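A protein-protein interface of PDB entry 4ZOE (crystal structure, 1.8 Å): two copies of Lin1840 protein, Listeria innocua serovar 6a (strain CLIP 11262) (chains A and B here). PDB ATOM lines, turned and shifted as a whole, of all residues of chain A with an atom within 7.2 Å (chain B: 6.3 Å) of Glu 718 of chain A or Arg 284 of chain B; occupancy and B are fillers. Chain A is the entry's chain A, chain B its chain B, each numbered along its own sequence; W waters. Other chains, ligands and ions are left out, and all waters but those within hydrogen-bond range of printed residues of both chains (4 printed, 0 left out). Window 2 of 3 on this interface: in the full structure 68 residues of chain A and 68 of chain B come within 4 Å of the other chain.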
ATOM      1  N   PRO A 615      10.479   1.899 -11.220  1.00  0.00           N
ATOM      2  CA  PRO A 615      11.053   1.110 -12.327  1.00  0.00           C
ATOM      3  C   PRO A 615      12.426   1.577 -12.785  1.00  0.00           C
ATOM      4  O   PRO A 615      12.737   2.751 -12.784  1.00  0.00           O
ATOM      5  CB  PRO A 615      10.047   1.305 -13.483  1.00  0.00           C
ATOM      6  CG  PRO A 615       9.084   2.368 -13.035  1.00  0.00           C
ATOM      7  CD  PRO A 615       9.139   2.436 -11.552  1.00  0.00           C
ATOM      8  N   LYS A 616      13.253   0.652 -13.174  1.00  0.00           N
ATOM      9  CA  LYS A 616      14.512   0.998 -13.784  1.00  0.00           C
ATOM     10  C   LYS A 616      14.354   1.271 -15.287  1.00  0.00           C
ATOM     11  O   LYS A 616      15.242   1.880 -15.889  1.00  0.00           O
ATOM     12  CB  LYS A 616      15.558  -0.076 -13.510  1.00  0.00           C
ATOM     13  CG  LYS A 616      16.866   0.153 -14.232  1.00  0.00           C
ATOM     14  CD  LYS A 616      17.610   1.445 -13.838  1.00  0.00           C
ATOM     15  CE  LYS A 616      18.232   2.117 -15.049  1.00  0.00           C
ATOM     16  NZ  LYS A 616      19.483   2.862 -14.695  1.00  0.00           N
ATOM     17  N   GLU A 617      13.220   0.881 -15.882  1.00  0.00           N
ATOM     18  CA  GLU A 617      12.982   1.136 -17.286  1.00  0.00           C
ATOM     19  C   GLU A 617      11.556   1.501 -17.537  1.00  0.00           C
ATOM     20  O   GLU A 617      10.686   1.160 -16.743  1.00  0.00           O
ATOM     21  CB  GLU A 617      13.305  -0.062 -18.106  1.00  0.00           C
ATOM     22  CG  GLU A 617      14.704  -0.528 -17.829  1.00  0.00           C
ATOM     23  CD  GLU A 617      15.256  -1.334 -18.964  1.00  0.00           C
ATOM     24  OE1 GLU A 617      15.589  -0.705 -19.993  1.00  0.00           O
ATOM     25  OE2 GLU A 617      15.318  -2.569 -18.855  1.00  0.00           O
ATOM     26  N   LEU A 618      11.338   2.108 -18.684  1.00  0.00           N
ATOM     27  CA  LEU A 618      10.098   2.689 -19.032  1.00  0.00           C
ATOM     28  C   LEU A 618      10.088   2.668 -20.553  1.00  0.00           C
ATOM     29  O   LEU A 618      11.174   2.795 -21.223  1.00  0.00           O
ATOM     30  CB  LEU A 618      10.113   4.126 -18.526  1.00  0.00           C
ATOM     31  CG  LEU A 618       8.815   4.776 -18.188  1.00  0.00           C
ATOM     32  CD1 LEU A 618       7.976   3.863 -17.286  1.00  0.00           C
ATOM     33  CD2 LEU A 618       9.100   6.083 -17.410  1.00  0.00           C
ATOM     34  N   ASN A 619       8.928   2.394 -21.119  1.00  0.00           N
ATOM     35  CA  ASN A 619       8.776   2.501 -22.570  1.00  0.00           C
ATOM     36  C   ASN A 619       8.603   3.969 -22.981  1.00  0.00           C
ATOM     37  O   ASN A 619       8.209   4.787 -22.203  1.00  0.00           O
ATOM     38  CB  ASN A 619       7.584   1.671 -23.055  1.00  0.00           C
ATOM     39  CG  ASN A 619       7.867   0.175 -22.980  1.00  0.00           C
ATOM     40  OD1 ASN A 619       7.260  -0.505 -22.208  1.00  0.00           O
ATOM     41  ND2 ASN A 619       8.822  -0.304 -23.750  1.00  0.00           N
ATOM     42  N   VAL A 649      19.440  13.332 -19.215  1.00  0.00           N
ATOM     43  CA  VAL A 649      20.913  13.339 -19.096  1.00  0.00           C
ATOM     44  C   VAL A 649      21.675  13.649 -20.365  1.00  0.00           C
ATOM     45  O   VAL A 649      22.625  14.419 -20.313  1.00  0.00           O
ATOM     46  CB  VAL A 649      21.419  12.064 -18.413  1.00  0.00           C
ATOM     47  CG1 VAL A 649      22.896  12.068 -18.378  1.00  0.00           C
ATOM     48  CG2 VAL A 649      20.799  11.989 -17.020  1.00  0.00           C
ATOM     49  N   THR A 650      21.264  13.041 -21.487  1.00  0.00           N
ATOM     50  CA  THR A 650      21.864  13.201 -22.816  1.00  0.00           C
ATOM     51  C   THR A 650      20.766  13.407 -23.818  1.00  0.00           C
ATOM     52  O   THR A 650      19.775  12.698 -23.809  1.00  0.00           O
ATOM     53  CB  THR A 650      22.682  11.975 -23.156  1.00  0.00           C
ATOM     54  OG1 THR A 650      23.528  11.663 -22.032  1.00  0.00           O
ATOM     55  CG2 THR A 650      23.485  12.142 -24.452  1.00  0.00           C
ATOM     56  N   ALA A 651      20.880  14.467 -24.621  1.00  0.00           N
ATOM     57  CA  ALA A 651      19.891  14.781 -25.566  1.00  0.00           C
ATOM     58  C   ALA A 651      20.433  15.447 -26.819  1.00  0.00           C
ATOM     59  O   ALA A 651      21.565  15.888 -26.862  1.00  0.00           O
ATOM     60  CB  ALA A 651      18.814  15.624 -24.862  1.00  0.00           C
ATOM     61  N   PRO A 698      14.681   8.189 -26.592  1.00  0.00           N
ATOM     62  CA  PRO A 698      15.062   7.161 -25.666  1.00  0.00           C
ATOM     63  C   PRO A 698      16.366   7.565 -24.958  1.00  0.00           C
ATOM     64  O   PRO A 698      17.193   8.288 -25.567  1.00  0.00           O
ATOM     65  CB  PRO A 698      15.245   5.905 -26.574  1.00  0.00           C
ATOM     66  CG  PRO A 698      15.420   6.420 -27.955  1.00  0.00           C
ATOM     67  CD  PRO A 698      14.832   7.803 -28.018  1.00  0.00           C
ATOM     68  N   GLY A 699      16.534   7.085 -23.724  1.00  0.00           N
ATOM     69  CA  GLY A 699      17.741   7.322 -22.960  1.00  0.00           C
ATOM     70  C   GLY A 699      17.513   7.488 -21.458  1.00  0.00           C
ATOM     71  O   GLY A 699      16.353   7.300 -20.939  1.00  0.00           O
ATOM     72  N   LEU A 700      18.598   7.854 -20.752  1.00  0.00           N
ATOM     73  CA  LEU A 700      18.619   7.955 -19.290  1.00  0.00           C
ATOM     74  C   LEU A 700      17.998   9.269 -18.825  1.00  0.00           C
ATOM     75  O   LEU A 700      18.424  10.312 -19.312  1.00  0.00           O
ATOM     76  CB  LEU A 700      20.087   7.905 -18.804  1.00  0.00           C
ATOM     77  CG  LEU A 700      20.298   7.927 -17.289  1.00  0.00           C
ATOM     78  CD1 LEU A 700      19.700   6.693 -16.611  1.00  0.00           C
ATOM     79  CD2 LEU A 700      21.758   8.044 -16.848  1.00  0.00           C
ATOM     80  N   HIS A 701      17.046   9.197 -17.878  1.00  0.00           N
ATOM     81  CA  HIS A 701      16.560  10.319 -17.103  1.00  0.00           C
ATOM     82  C   HIS A 701      16.861  10.137 -15.612  1.00  0.00           C
ATOM     83  O   HIS A 701      16.944   8.994 -15.072  1.00  0.00           O
ATOM     84  CB  HIS A 701      15.028  10.477 -17.333  1.00  0.00           C
ATOM     85  CG  HIS A 701      14.707  10.891 -18.723  1.00  0.00           C
ATOM     86  ND1 HIS A 701      14.346  12.174 -19.074  1.00  0.00           N
ATOM     87  CD2 HIS A 701      14.786  10.198 -19.873  1.00  0.00           C
ATOM     88  CE1 HIS A 701      14.256  12.250 -20.389  1.00  0.00           C
ATOM     89  NE2 HIS A 701      14.446  11.045 -20.890  1.00  0.00           N
ATOM     90  N   GLU A 716      17.353   6.766 -11.126  1.00  0.00           N
ATOM     91  CA  GLU A 716      17.676   6.702 -12.571  1.00  0.00           C
ATOM     92  C   GLU A 716      16.677   5.831 -13.200  1.00  0.00           C
ATOM     93  O   GLU A 716      16.314   4.794 -12.616  1.00  0.00           O
ATOM     94  CB  GLU A 716      19.101   6.191 -12.871  1.00  0.00           C
ATOM     95  CG  GLU A 716      20.039   7.326 -12.417  1.00  0.00           C
ATOM     96  CD  GLU A 716      21.488   7.217 -12.739  1.00  0.00           C
ATOM     97  OE1 GLU A 716      21.912   6.218 -13.304  1.00  0.00           O
ATOM     98  OE2 GLU A 716      22.190   8.194 -12.350  1.00  0.00           O
ATOM     99  N   VAL A 717      16.192   6.280 -14.367  1.00  0.00           N
ATOM    100  CA  VAL A 717      15.194   5.512 -15.223  1.00  0.00           C
ATOM    101  C   VAL A 717      15.662   5.520 -16.672  1.00  0.00           C
ATOM    102  O   VAL A 717      15.836   6.587 -17.232  1.00  0.00           O
ATOM    103  CB  VAL A 717      13.779   6.149 -15.220  1.00  0.00           C
ATOM    104  CG1 VAL A 717      12.834   5.238 -15.945  1.00  0.00           C
ATOM    105  CG2 VAL A 717      13.240   6.285 -13.846  1.00  0.00           C
ATOM    106  N   GLU A 718      15.918   4.358 -17.278  1.00  0.00           N
ATOM    107  CA  GLU A 718      16.312   4.273 -18.672  1.00  0.00           C
ATOM    108  C   GLU A 718      15.047   4.167 -19.541  1.00  0.00           C
ATOM    109  O   GLU A 718      14.261   3.223 -19.404  1.00  0.00           O
ATOM    110  CB  GLU A 718      17.261   3.124 -18.921  1.00  0.00           C
ATOM    111  CG  GLU A 718      17.826   3.071 -20.342  1.00  0.00           C
ATOM    112  CD  GLU A 718      18.901   4.116 -20.650  1.00  0.00           C
ATOM    113  OE1 GLU A 718      19.038   4.476 -21.849  1.00  0.00           O
ATOM    114  OE2 GLU A 718      19.599   4.543 -19.730  1.00  0.00           O
ATOM    115  N   VAL A 719      14.860   5.133 -20.431  1.00  0.00           N
ATOM    116  CA  VAL A 719      13.667   5.194 -21.311  1.00  0.00           C
ATOM    117  C   VAL A 719      14.011   4.617 -22.671  1.00  0.00           C
ATOM    118  O   VAL A 719      15.023   5.010 -23.317  1.00  0.00           O
ATOM    119  CB  VAL A 719      13.028   6.621 -21.332  1.00  0.00           C
ATOM    120  CG1 VAL A 719      11.769   6.660 -22.171  1.00  0.00           C
ATOM    121  CG2 VAL A 719      12.632   7.042 -19.936  1.00  0.00           C
ATOM    122  N   GLY A 720      13.270   3.576 -23.111  1.00  0.00           N
ATOM    123  CA  GLY A 720      13.382   3.179 -24.509  1.00  0.00           C
ATOM    124  C   GLY A 720      12.399   2.158 -25.047  1.00  0.00           C
ATOM    125  O   GLY A 720      11.328   2.025 -24.542  1.00  0.00           O
ATOM    126  N   GLY A 721      12.782   1.423 -26.081  1.00  0.00           N
ATOM    127  CA  GLY A 721      11.922   0.295 -26.549  1.00  0.00           C
ATOM    128  C   GLY A 721      10.854   0.736 -27.498  1.00  0.00           C
ATOM    129  O   GLY A 721      11.092   1.509 -28.406  1.00  0.00           O
ATOM    130  N   ILE B 278      30.132  15.901 -24.015  1.00  0.00           N
ATOM    131  CA  ILE B 278      29.619  14.987 -22.974  1.00  0.00           C
ATOM    132  C   ILE B 278      29.115  15.724 -21.734  1.00  0.00           C
ATOM    133  O   ILE B 278      27.935  15.576 -21.328  1.00  0.00           O
ATOM    134  CB  ILE B 278      30.619  13.838 -22.598  1.00  0.00           C
ATOM    135  CG1 ILE B 278      30.986  13.074 -23.830  1.00  0.00           C
ATOM    136  CG2 ILE B 278      30.035  12.987 -21.489  1.00  0.00           C
ATOM    137  CD1 ILE B 278      32.383  12.456 -23.767  1.00  0.00           C
ATOM    138  N   GLY B 281      25.956  17.450 -22.048  1.00  0.00           N
ATOM    139  CA  GLY B 281      24.744  16.581 -22.118  1.00  0.00           C
ATOM    140  C   GLY B 281      24.265  16.369 -23.564  1.00  0.00           C
ATOM    141  O   GLY B 281      23.101  16.064 -23.779  1.00  0.00           O
ATOM    142  N   THR B 282      25.134  16.431 -24.567  1.00  0.00           N
ATOM    143  CA  THR B 282      24.692  16.130 -25.919  1.00  0.00           C
ATOM    144  C   THR B 282      25.438  14.978 -26.644  1.00  0.00           C
ATOM    145  O   THR B 282      25.281  14.769 -27.854  1.00  0.00           O
ATOM    146  CB  THR B 282      24.699  17.432 -26.784  1.00  0.00           C
ATOM    147  OG1 THR B 282      26.026  17.996 -26.867  1.00  0.00           O
ATOM    148  CG2 THR B 282      23.710  18.476 -26.248  1.00  0.00           C
ATOM    149  N   ALA B 283      26.288  14.313 -25.895  1.00  0.00           N
ATOM    150  CA  ALA B 283      26.873  13.020 -26.257  1.00  0.00           C
ATOM    151  C   ALA B 283      26.949  12.161 -25.003  1.00  0.00           C
ATOM    152  O   ALA B 283      27.191  12.654 -23.888  1.00  0.00           O
ATOM    153  CB  ALA B 283      28.216  13.199 -26.887  1.00  0.00           C
ATOM    154  N   ARG B 284      26.637  10.878 -25.136  1.00  0.00           N
ATOM    155  CA  ARG B 284      26.588  10.040 -23.959  1.00  0.00           C
ATOM    156  C   ARG B 284      28.011   9.647 -23.523  1.00  0.00           C
ATOM    157  O   ARG B 284      28.256   9.397 -22.380  1.00  0.00           O
ATOM    158  CB  ARG B 284      25.592   8.792 -24.185  1.00  0.00           C
ATOM    159  CG  ARG B 284      25.440   7.812 -23.025  1.00  0.00           C
ATOM    160  CD  ARG B 284      24.245   6.844 -23.283  1.00  0.00           C
ATOM    161  NE  ARG B 284      23.827   6.316 -22.002  1.00  0.00           N
ATOM    162  CZ  ARG B 284      22.628   5.748 -21.691  1.00  0.00           C
ATOM    163  NH1 ARG B 284      21.652   5.636 -22.575  1.00  0.00           N
ATOM    164  NH2 ARG B 284      22.421   5.260 -20.471  1.00  0.00           N
ATOM    165  N   ASN B 285      28.952   9.668 -24.411  1.00  0.00           N
ATOM    166  CA  ASN B 285      30.302   9.043 -24.139  1.00  0.00           C
ATOM    167  C   ASN B 285      31.271   9.487 -25.209  1.00  0.00           C
ATOM    168  O   ASN B 285      30.847  10.153 -26.120  1.00  0.00           O
ATOM    169  CB  ASN B 285      30.189   7.525 -24.146  1.00  0.00           C
ATOM    170  CG  ASN B 285      29.465   7.004 -25.341  1.00  0.00           C
ATOM    171  OD1 ASN B 285      29.614   7.483 -26.449  1.00  0.00           O
ATOM    172  ND2 ASN B 285      28.610   6.009 -25.107  1.00  0.00           N
ATOM    173  N   PRO B 286      32.596   9.108 -25.127  1.00  0.00           N
ATOM    174  CA  PRO B 286      33.540   9.583 -26.146  1.00  0.00           C
ATOM    175  C   PRO B 286      33.269   9.032 -27.560  1.00  0.00           C
ATOM    176  O   PRO B 286      33.583   9.681 -28.547  1.00  0.00           O
ATOM    177  CB  PRO B 286      34.878   9.132 -25.586  1.00  0.00           C
ATOM    178  CG  PRO B 286      34.668   9.109 -24.062  1.00  0.00           C
ATOM    179  CD  PRO B 286      33.279   8.605 -23.917  1.00  0.00           C
ATOM    180  N   GLU B 288      30.265   8.821 -28.972  1.00  0.00           N
ATOM    181  CA  GLU B 288      29.285   9.730 -29.581  1.00  0.00           C
ATOM    182  C   GLU B 288      29.890  11.093 -29.873  1.00  0.00           C
ATOM    183  O   GLU B 288      29.645  11.671 -30.899  1.00  0.00           O
ATOM    184  CB  GLU B 288      28.026   9.887 -28.707  1.00  0.00           C
ATOM    185  CG  GLU B 288      27.172   8.637 -28.685  1.00  0.00           C
ATOM    186  CD  GLU B 288      25.815   8.792 -28.026  1.00  0.00           C
ATOM    187  OE1 GLU B 288      25.509   9.895 -27.453  1.00  0.00           O
ATOM    188  OE2 GLU B 288      25.051   7.762 -28.087  1.00  0.00           O
ATOM    189  N   ALA B 289      30.638  11.615 -28.938  1.00  0.00           N
ATOM    190  CA  ALA B 289      31.368  12.905 -29.126  1.00  0.00           C
ATOM    191  C   ALA B 289      32.237  12.886 -30.356  1.00  0.00           C
ATOM    192  O   ALA B 289      32.187  13.791 -31.158  1.00  0.00           O
ATOM    193  CB  ALA B 289      32.153  13.266 -27.882  1.00  0.00           C
ATOM    194  N   PHE B 292      29.784  12.765 -33.436  1.00  0.00           N
ATOM    195  CA  PHE B 292      29.053  13.973 -33.694  1.00  0.00           C
ATOM    196  C   PHE B 292      29.989  15.119 -34.143  1.00  0.00           C
ATOM    197  O   PHE B 292      29.664  15.932 -35.031  1.00  0.00           O
ATOM    198  CB  PHE B 292      28.158  14.339 -32.486  1.00  0.00           C
ATOM    199  CG  PHE B 292      27.186  13.274 -32.064  1.00  0.00           C
ATOM    200  CD1 PHE B 292      26.618  12.397 -32.990  1.00  0.00           C
ATOM    201  CD2 PHE B 292      26.690  13.270 -30.762  1.00  0.00           C
ATOM    202  CE1 PHE B 292      25.659  11.483 -32.569  1.00  0.00           C
ATOM    203  CE2 PHE B 292      25.779  12.316 -30.324  1.00  0.00           C
ATOM    204  CZ  PHE B 292      25.243  11.428 -31.239  1.00  0.00           C
HETATM  205  O   HOH W   1      21.135  17.007 -21.903  1.00  0.00           O
HETATM  206  O   HOH W   2      25.837  13.060 -21.607  1.00  0.00           O
HETATM  207  O   HOH W   3      23.083  14.534 -29.259  1.00  0.00           O
HETATM  208  O   HOH W   4      20.873   8.967 -22.196  1.00  0.00           O
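The backbone NH of Ala 651 of chain A lies within hydrogen-bond range of the backbone carbonyl oxygen of Gly 281 of chain B, 2.9 Å away. NH1 of Arg 284 of chain B is in salt-bridge range of OE1 of Glu 718 of chain A.
The backbone carbonyl oxygen (O) of Lys 616 of chain A sits at hydrogen-bond distance from the backbone NH (N) of Glu 718 of chain A, at 2.9 Å. The backbone carbonyl oxygen (O) of Glu 718 of chain A is in hydrogen-bond range of the backbone NH (N) of Leu 618 of chain A. The backbone NH (N) of Val 649 of chain A sits at hydrogen-bond distance from the backbone carbonyl oxygen (O) of Leu 700 of chain A (3.2 Å). The backbone NH (N) of Arg 284 of chain B lies within hydrogen-bond range of the side-chain carboxylate (OE1) of Glu 288 of chain B (2.8 Å).
Val 649 of chain A touches Gly 281 of chain B. Gly 281 of chain B touches Thr 650 of chain A. Thr 650 of chain A touches Ala 283 of chain B (CG2 to C, 3.5 Å). Thr 650 of chain A touches Arg 284 of chain B (CG2 to N, 3.5 Å). Ala 651 of chain A touches Thr 282 of chain B (O to CA, 3.3 Å). Leu 700 of chain A touches Arg 284 of chain B.
Of chain B, only Arg 284 comes within 4 Å of Glu 718 of chain A. Of chain A, only Thr 650 (3.5 Å), Leu 700 (3.9 Å) and Glu 718 (3.0 Å) come within 4 Å of Arg 284 of chain B. Printed residues of chain A within 4 Å of Gly 281 of chain B: Val 649, Thr 650 and Ala 651. Of the printed residues of chain A, Thr 282 of chain B touches Ala 651. The nearest printed residue of chain B that does not touch Glu 718 of chain A is Glu 288 of chain B (9.3 Å). The nearest printed residue of chain A that does not touch Ala 283 of chain B is Ala 651 of chain A (5.1 Å).
Of the 18 printed residues of chain A, 5 touch a printed residue of chain B. Printed residues of chain A that touch a printed residue of chain B: Val 649, Thr 650, Ala 651, Leu 700 and Glu 718. Hydrophobic or aromatic side chains of chain A within 4 Å of the printed part of chain B: Leu 700. Along chain A the printed residues that touch a printed residue of chain B span positions 649 to 718. Among the printed residues, Asp or Glu carboxylates within 4 Å of a Lys or Arg side-chain nitrogen of the other chain: Glu 718 of chain A with Arg 284 of chain B.
No position is printed for both chains.
Water W3 lies within hydrogen-bond range of O of Thr 282 of chain B and O of Ala 651 of chain A. Water W2 lies within hydrogen-bond range of the backbone carbonyl oxygen of Ala 283 of chain B (2.7 Å), the side-chain hydroxyl of Thr 650 of chain A (2.7 Å) and the backbone carbonyl oxygen of Ile 278 of chain B (3.3 Å). Water W1 bridges O of Gly 281 of chain B (2.9 Å) and O of Val 649 of chain A (3.4 Å). Water W4 lies within hydrogen-bond range of the backbone NH of Leu 700 of chain A (2.9 Å) and the guanidinium group of Arg 284 of chain B (3.4 Å).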
